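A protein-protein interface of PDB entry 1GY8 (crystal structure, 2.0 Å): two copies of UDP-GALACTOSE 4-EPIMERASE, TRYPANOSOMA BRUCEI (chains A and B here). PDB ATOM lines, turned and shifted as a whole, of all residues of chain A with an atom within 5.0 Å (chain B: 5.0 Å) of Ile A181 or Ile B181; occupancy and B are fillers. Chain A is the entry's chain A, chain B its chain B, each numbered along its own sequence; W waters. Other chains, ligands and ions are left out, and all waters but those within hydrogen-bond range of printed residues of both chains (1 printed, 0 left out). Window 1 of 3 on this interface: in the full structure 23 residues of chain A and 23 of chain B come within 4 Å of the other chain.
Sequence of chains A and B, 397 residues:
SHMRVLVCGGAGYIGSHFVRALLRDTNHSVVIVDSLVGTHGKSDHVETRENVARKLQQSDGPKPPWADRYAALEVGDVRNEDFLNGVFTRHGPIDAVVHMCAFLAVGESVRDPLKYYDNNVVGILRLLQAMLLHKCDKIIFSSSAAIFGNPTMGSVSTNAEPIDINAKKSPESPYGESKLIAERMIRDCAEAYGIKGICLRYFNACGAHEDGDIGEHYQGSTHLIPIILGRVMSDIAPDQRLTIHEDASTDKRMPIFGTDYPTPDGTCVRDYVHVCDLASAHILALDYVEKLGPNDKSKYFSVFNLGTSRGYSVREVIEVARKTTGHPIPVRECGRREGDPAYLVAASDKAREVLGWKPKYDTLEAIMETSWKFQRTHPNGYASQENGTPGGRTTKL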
ATOM      1  N   TYR A 117      21.683 -16.190 -18.596  1.00  0.00           N
ATOM      2  CA  TYR A 117      20.505 -15.829 -17.818  1.00  0.00           C
ATOM      3  C   TYR A 117      20.220 -16.929 -16.791  1.00  0.00           C
ATOM      4  O   TYR A 117      19.858 -16.651 -15.653  1.00  0.00           O
ATOM      5  CB  TYR A 117      19.293 -15.626 -18.729  1.00  0.00           C
ATOM      6  CG  TYR A 117      19.299 -14.288 -19.441  1.00  0.00           C
ATOM      7  CD1 TYR A 117      19.211 -13.095 -18.720  1.00  0.00           C
ATOM      8  CD2 TYR A 117      19.406 -14.210 -20.834  1.00  0.00           C
ATOM      9  CE1 TYR A 117      19.228 -11.857 -19.367  1.00  0.00           C
ATOM     10  CE2 TYR A 117      19.428 -12.979 -21.490  1.00  0.00           C
ATOM     11  CZ  TYR A 117      19.337 -11.807 -20.754  1.00  0.00           C
ATOM     12  OH  TYR A 117      19.347 -10.586 -21.392  1.00  0.00           O
ATOM     13  N   VAL A 121      21.244 -15.349 -13.358  1.00  0.00           N
ATOM     14  CA  VAL A 121      20.019 -14.886 -12.715  1.00  0.00           C
ATOM     15  C   VAL A 121      19.398 -15.907 -11.766  1.00  0.00           C
ATOM     16  O   VAL A 121      18.950 -15.543 -10.680  1.00  0.00           O
ATOM     17  CB  VAL A 121      18.973 -14.445 -13.759  1.00  0.00           C
ATOM     18  CG1 VAL A 121      17.777 -13.821 -13.062  1.00  0.00           C
ATOM     19  CG2 VAL A 121      19.590 -13.443 -14.722  1.00  0.00           C
ATOM     20  N   GLU A 177      23.147  -7.634 -18.814  1.00  0.00           N
ATOM     21  CA  GLU A 177      21.731  -7.677 -18.436  1.00  0.00           C
ATOM     22  C   GLU A 177      21.514  -8.552 -17.207  1.00  0.00           C
ATOM     23  O   GLU A 177      20.712  -8.220 -16.345  1.00  0.00           O
ATOM     24  CB  GLU A 177      20.872  -8.236 -19.578  1.00  0.00           C
ATOM     25  CG  GLU A 177      20.849  -7.395 -20.844  1.00  0.00           C
ATOM     26  CD  GLU A 177      20.007  -6.140 -20.708  1.00  0.00           C
ATOM     27  OE1 GLU A 177      19.424  -5.915 -19.622  1.00  0.00           O
ATOM     28  OE2 GLU A 177      19.924  -5.379 -21.695  1.00  0.00           O
ATOM     29  N   SER A 178      22.221  -9.678 -17.150  1.00  0.00           N
ATOM     30  CA  SER A 178      22.093 -10.618 -16.042  1.00  0.00           C
ATOM     31  C   SER A 178      22.589 -10.027 -14.729  1.00  0.00           C
ATOM     32  O   SER A 178      22.052 -10.342 -13.665  1.00  0.00           O
ATOM     33  CB  SER A 178      22.843 -11.924 -16.346  1.00  0.00           C
ATOM     34  OG  SER A 178      24.250 -11.755 -16.326  1.00  0.00           O
ATOM     35  N   LYS A 179      23.612  -9.178 -14.804  1.00  0.00           N
ATOM     36  CA  LYS A 179      24.153  -8.537 -13.612  1.00  0.00           C
ATOM     37  C   LYS A 179      23.208  -7.439 -13.151  1.00  0.00           C
ATOM     38  O   LYS A 179      23.009  -7.239 -11.950  1.00  0.00           O
ATOM     39  CB  LYS A 179      25.537  -7.935 -13.889  1.00  0.00           C
ATOM     40  CG  LYS A 179      26.659  -8.947 -14.003  1.00  0.00           C
ATOM     41  CD  LYS A 179      26.793  -9.747 -12.712  1.00  0.00           C
ATOM     42  CE  LYS A 179      27.979 -10.691 -12.755  1.00  0.00           C
ATOM     43  NZ  LYS A 179      28.051 -11.535 -11.521  1.00  0.00           N
ATOM     44  N   LEU A 180      22.621  -6.735 -14.112  1.00  0.00           N
ATOM     45  CA  LEU A 180      21.698  -5.652 -13.808  1.00  0.00           C
ATOM     46  C   LEU A 180      20.413  -6.157 -13.149  1.00  0.00           C
ATOM     47  O   LEU A 180      19.948  -5.574 -12.173  1.00  0.00           O
ATOM     48  CB  LEU A 180      21.367  -4.870 -15.087  1.00  0.00           C
ATOM     49  CG  LEU A 180      20.417  -3.673 -14.944  1.00  0.00           C
ATOM     50  CD1 LEU A 180      20.959  -2.694 -13.898  1.00  0.00           C
ATOM     51  CD2 LEU A 180      20.261  -2.981 -16.297  1.00  0.00           C
ATOM     52  N   ILE A 181      19.835  -7.237 -13.672  1.00  0.00           N
ATOM     53  CA  ILE A 181      18.611  -7.764 -13.083  1.00  0.00           C
ATOM     54  C   ILE A 181      18.888  -8.260 -11.661  1.00  0.00           C
ATOM     55  O   ILE A 181      18.034  -8.151 -10.780  1.00  0.00           O
ATOM     56  CB  ILE A 181      17.991  -8.911 -13.937  1.00  0.00           C
ATOM     57  CG1 ILE A 181      16.642  -9.323 -13.348  1.00  0.00           C
ATOM     58  CG2 ILE A 181      18.901 -10.102 -13.968  1.00  0.00           C
ATOM     59  CD1 ILE A 181      15.600  -8.204 -13.321  1.00  0.00           C
ATOM     60  N   ALA A 182      20.084  -8.791 -11.432  1.00  0.00           N
ATOM     61  CA  ALA A 182      20.444  -9.251 -10.096  1.00  0.00           C
ATOM     62  C   ALA A 182      20.424  -8.067  -9.117  1.00  0.00           C
ATOM     63  O   ALA A 182      19.977  -8.210  -7.978  1.00  0.00           O
ATOM     64  CB  ALA A 182      21.821  -9.895 -10.112  1.00  0.00           C
ATOM     65  N   GLU A 183      20.908  -6.903  -9.553  1.00  0.00           N
ATOM     66  CA  GLU A 183      20.910  -5.713  -8.692  1.00  0.00           C
ATOM     67  C   GLU A 183      19.487  -5.277  -8.354  1.00  0.00           C
ATOM     68  O   GLU A 183      19.210  -4.866  -7.227  1.00  0.00           O
ATOM     69  CB  GLU A 183      21.656  -4.547  -9.356  1.00  0.00           C
ATOM     70  CG  GLU A 183      23.169  -4.720  -9.388  1.00  0.00           C
ATOM     71  CD  GLU A 183      23.910  -3.424  -9.668  1.00  0.00           C
ATOM     72  OE1 GLU A 183      23.292  -2.344  -9.557  1.00  0.00           O
ATOM     73  OE2 GLU A 183      25.117  -3.484  -9.983  1.00  0.00           O
ATOM     74  N   ARG A 184      18.587  -5.368  -9.333  1.00  0.00           N
ATOM     75  CA  ARG A 184      17.183  -4.998  -9.132  1.00  0.00           C
ATOM     76  C   ARG A 184      16.545  -5.954  -8.126  1.00  0.00           C
ATOM     77  O   ARG A 184      15.783  -5.533  -7.267  1.00  0.00           O
ATOM     78  CB  ARG A 184      16.391  -5.089 -10.443  1.00  0.00           C
ATOM     79  CG  ARG A 184      16.960  -4.314 -11.610  1.00  0.00           C
ATOM     80  CD  ARG A 184      17.190  -2.873 -11.253  1.00  0.00           C
ATOM     81  NE  ARG A 184      17.481  -2.071 -12.434  1.00  0.00           N
ATOM     82  CZ  ARG A 184      18.028  -0.861 -12.396  1.00  0.00           C
ATOM     83  NH1 ARG A 184      18.353  -0.315 -11.229  1.00  0.00           N
ATOM     84  NH2 ARG A 184      18.233  -0.190 -13.523  1.00  0.00           N
ATOM     85  N   MET A 185      16.864  -7.243  -8.243  1.00  0.00           N
ATOM     86  CA  MET A 185      16.308  -8.261  -7.343  1.00  0.00           C
ATOM     87  C   MET A 185      16.786  -8.045  -5.908  1.00  0.00           C
ATOM     88  O   MET A 185      16.008  -8.123  -4.963  1.00  0.00           O
ATOM     89  CB  MET A 185      16.716  -9.659  -7.814  1.00  0.00           C
ATOM     90  CG  MET A 185      16.103 -10.082  -9.147  1.00  0.00           C
ATOM     91  SD  MET A 185      16.775 -11.652  -9.741  1.00  0.00           S
ATOM     92  CE  MET A 185      16.309 -12.760  -8.405  1.00  0.00           C
ATOM     93  N   TYR B 117       9.977 -12.929  -9.138  1.00  0.00           N
ATOM     94  CA  TYR B 117      11.150 -13.130  -9.970  1.00  0.00           C
ATOM     95  C   TYR B 117      11.266 -14.611 -10.311  1.00  0.00           C
ATOM     96  O   TYR B 117      11.597 -14.970 -11.439  1.00  0.00           O
ATOM     97  CB  TYR B 117      12.414 -12.638  -9.256  1.00  0.00           C
ATOM     98  CG  TYR B 117      12.582 -11.133  -9.310  1.00  0.00           C
ATOM     99  CD1 TYR B 117      12.771 -10.478 -10.524  1.00  0.00           C
ATOM    100  CD2 TYR B 117      12.546 -10.362  -8.145  1.00  0.00           C
ATOM    101  CE1 TYR B 117      12.923  -9.089 -10.583  1.00  0.00           C
ATOM    102  CE2 TYR B 117      12.699  -8.975  -8.192  1.00  0.00           C
ATOM    103  CZ  TYR B 117      12.888  -8.347  -9.415  1.00  0.00           C
ATOM    104  OH  TYR B 117      13.058  -6.980  -9.463  1.00  0.00           O
ATOM    105  N   VAL B 121      10.293 -14.850 -14.094  1.00  0.00           N
ATOM    106  CA  VAL B 121      11.533 -14.916 -14.851  1.00  0.00           C
ATOM    107  C   VAL B 121      12.000 -16.335 -15.148  1.00  0.00           C
ATOM    108  O   VAL B 121      12.451 -16.614 -16.254  1.00  0.00           O
ATOM    109  CB  VAL B 121      12.667 -14.131 -14.144  1.00  0.00           C
ATOM    110  CG1 VAL B 121      13.899 -14.079 -15.030  1.00  0.00           C
ATOM    111  CG2 VAL B 121      12.192 -12.716 -13.830  1.00  0.00           C
ATOM    112  N   GLU B 177       9.492  -5.271 -13.262  1.00  0.00           N
ATOM    113  CA  GLU B 177      10.878  -5.662 -13.534  1.00  0.00           C
ATOM    114  C   GLU B 177      10.951  -7.058 -14.151  1.00  0.00           C
ATOM    115  O   GLU B 177      11.766  -7.299 -15.042  1.00  0.00           O
ATOM    116  CB  GLU B 177      11.707  -5.673 -12.249  1.00  0.00           C
ATOM    117  CG  GLU B 177      11.877  -4.326 -11.573  1.00  0.00           C
ATOM    118  CD  GLU B 177      12.853  -3.419 -12.297  1.00  0.00           C
ATOM    119  OE1 GLU B 177      13.420  -3.834 -13.332  1.00  0.00           O
ATOM    120  OE2 GLU B 177      13.059  -2.282 -11.821  1.00  0.00           O
ATOM    121  N   SER B 178      10.108  -7.968 -13.660  1.00  0.00           N
ATOM    122  CA  SER B 178      10.090  -9.343 -14.144  1.00  0.00           C
ATOM    123  C   SER B 178       9.612  -9.432 -15.589  1.00  0.00           C
ATOM    124  O   SER B 178      10.066 -10.292 -16.338  1.00  0.00           O
ATOM    125  CB  SER B 178       9.204 -10.228 -13.246  1.00  0.00           C
ATOM    126  OG  SER B 178       7.824  -9.917 -13.365  1.00  0.00           O
ATOM    127  N   LYS B 179       8.690  -8.552 -15.967  1.00  0.00           N
ATOM    128  CA  LYS B 179       8.173  -8.529 -17.328  1.00  0.00           C
ATOM    129  C   LYS B 179       9.211  -7.919 -18.259  1.00  0.00           C
ATOM    130  O   LYS B 179       9.375  -8.357 -19.396  1.00  0.00           O
ATOM    131  CB  LYS B 179       6.877  -7.708 -17.411  1.00  0.00           C
ATOM    132  CG  LYS B 179       5.646  -8.396 -16.832  1.00  0.00           C
ATOM    133  CD  LYS B 179       5.382  -9.719 -17.540  1.00  0.00           C
ATOM    134  CE  LYS B 179       4.090 -10.364 -17.057  1.00  0.00           C
ATOM    135  NZ  LYS B 179       3.857 -11.689 -17.707  1.00  0.00           N
ATOM    136  N   LEU B 180       9.911  -6.902 -17.766  1.00  0.00           N
ATOM    137  CA  LEU B 180      10.931  -6.230 -18.556  1.00  0.00           C
ATOM    138  C   LEU B 180      12.128  -7.138 -18.846  1.00  0.00           C
ATOM    139  O   LEU B 180      12.619  -7.172 -19.975  1.00  0.00           O
ATOM    140  CB  LEU B 180      11.391  -4.954 -17.838  1.00  0.00           C
ATOM    141  CG  LEU B 180      12.461  -4.108 -18.533  1.00  0.00           C
ATOM    142  CD1 LEU B 180      11.992  -3.716 -19.936  1.00  0.00           C
ATOM    143  CD2 LEU B 180      12.743  -2.872 -17.703  1.00  0.00           C
ATOM    144  N   ILE B 181      12.599  -7.876 -17.843  1.00  0.00           N
ATOM    145  CA  ILE B 181      13.735  -8.768 -18.065  1.00  0.00           C
ATOM    146  C   ILE B 181      13.344  -9.868 -19.051  1.00  0.00           C
ATOM    147  O   ILE B 181      14.169 -10.325 -19.837  1.00  0.00           O
ATOM    148  CB  ILE B 181      14.258  -9.401 -16.743  1.00  0.00           C
ATOM    149  CG1 ILE B 181      15.526 -10.212 -17.023  1.00  0.00           C
ATOM    150  CG2 ILE B 181      13.216 -10.307 -16.135  1.00  0.00           C
ATOM    151  CD1 ILE B 181      16.678  -9.386 -17.594  1.00  0.00           C
ATOM    152  N   ALA B 182      12.083 -10.286 -19.021  1.00  0.00           N
ATOM    153  CA  ALA B 182      11.619 -11.317 -19.946  1.00  0.00           C
ATOM    154  C   ALA B 182      11.732 -10.799 -21.384  1.00  0.00           C
ATOM    155  O   ALA B 182      12.124 -11.540 -22.285  1.00  0.00           O
ATOM    156  CB  ALA B 182      10.188 -11.698 -19.637  1.00  0.00           C
ATOM    157  N   GLU B 183      11.400  -9.525 -21.596  1.00  0.00           N
ATOM    158  CA  GLU B 183      11.493  -8.935 -22.933  1.00  0.00           C
ATOM    159  C   GLU B 183      12.939  -8.897 -23.430  1.00  0.00           C
ATOM    160  O   GLU B 183      13.204  -9.133 -24.611  1.00  0.00           O
ATOM    161  CB  GLU B 183      10.906  -7.519 -22.956  1.00  0.00           C
ATOM    162  CG  GLU B 183       9.389  -7.477 -22.882  1.00  0.00           C
ATOM    163  CD  GLU B 183       8.812  -6.136 -23.294  1.00  0.00           C
ATOM    164  OE1 GLU B 183       9.544  -5.331 -23.907  1.00  0.00           O
ATOM    165  OE2 GLU B 183       7.619  -5.889 -23.021  1.00  0.00           O
ATOM    166  N   ARG B 184      13.876  -8.604 -22.537  1.00  0.00           N
ATOM    167  CA  ARG B 184      15.272  -8.550 -22.928  1.00  0.00           C
ATOM    168  C   ARG B 184      15.811  -9.943 -23.216  1.00  0.00           C
ATOM    169  O   ARG B 184      16.655 -10.112 -24.091  1.00  0.00           O
ATOM    170  CB  ARG B 184      16.074  -7.837 -21.847  1.00  0.00           C
ATOM    171  CG  ARG B 184      15.518  -6.446 -21.620  1.00  0.00           C
ATOM    172  CD  ARG B 184      16.396  -5.588 -20.763  1.00  0.00           C
ATOM    173  NE  ARG B 184      15.839  -4.244 -20.630  1.00  0.00           N
ATOM    174  CZ  ARG B 184      16.451  -3.245 -20.000  1.00  0.00           C
ATOM    175  NH1 ARG B 184      17.645  -3.439 -19.445  1.00  0.00           N
ATOM    176  NH2 ARG B 184      15.869  -2.056 -19.921  1.00  0.00           N
ATOM    177  N   MET B 185      15.310 -10.945 -22.499  1.00  0.00           N
ATOM    178  CA  MET B 185      15.731 -12.322 -22.734  1.00  0.00           C
ATOM    179  C   MET B 185      15.228 -12.798 -24.096  1.00  0.00           C
ATOM    180  O   MET B 185      15.961 -13.433 -24.846  1.00  0.00           O
ATOM    181  CB  MET B 185      15.182 -13.244 -21.638  1.00  0.00           C
ATOM    182  CG  MET B 185      15.797 -13.019 -20.254  1.00  0.00           C
ATOM    183  SD  MET B 185      14.972 -13.997 -18.955  1.00  0.00           S
ATOM    184  CE  MET B 185      15.279 -15.659 -19.562  1.00  0.00           C
HETATM  185  O   HOH W   1      15.009  -1.977 -14.484  1.00  0.00           O
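OE1 of Glu A177 lies within salt-bridge range of NH1 of Arg B184, at 3.1 Å.
Ile B181 touches Tyr A117.
Arg B184 touches Tyr A117.
Tyr A117 touches Met B185 (CE1 to CG, 3.7 Å).
CD1 of Ile A181 touches CE1 of Tyr B117, 3.9 Å away.
Ile A181 touches Ile B181 (CD1 to CB, 3.9 Å).
OH of Tyr B117 touches O of Arg A184, at 3.8 Å.
Glu B177 touches Arg A184 (OE1 to CG, 3.97 Å).
CD1 of Tyr B117 touches CG of Met A185, at 3.6 Å.
Ile B181 touches just these residues of chain A: Tyr A117 and Ile A181.
Of the printed residues of chain B, Arg A184 touches Tyr B117 and Glu B177.
Of the printed residues of chain B, Tyr A117 touches Ile B181, Arg B184 and Met B185.
Of the printed residues of chain A, Met B185 touches Tyr A117 (3.7 Å).
Glu B183 touches none of the printed residues of chain A.
The nearest residue of chain B that does not touch Ile A181 is Glu B177 (4.3 Å).
The nearest printed residue of chain B that does not touch Tyr A117 is Val B121 (6.5 Å).
Tyr A117 touches Ile B181, and with the chains exchanged Ile A181 touches Tyr B117.
Tyr A117 touches Arg B184, and with the chains exchanged Arg A184 touches Tyr B117.
Tyr A117 touches Met B185, and with the chains exchanged Met A185 touches Tyr B117.
Glu A177 touches Arg B184, and with the chains exchanged Arg A184 touches Glu B177.
Hydrophobic or aromatic side chains of chain B that line the printed part of chain A: Tyr B117, Ile B181 and Met B185.
Hydrophobic or aromatic side chains of chain A that line the printed part of chain B: Tyr A117, Ile A181 and Met A185.
Among the printed residues, Asp or Glu carboxylates within 4 Å of a Lys or Arg side-chain nitrogen of the other chain: Glu A177 with Arg B184.
Water W1 lies within hydrogen-bond range of the side-chain carboxylate of Glu B177 and the guanidinium group of Arg A184.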
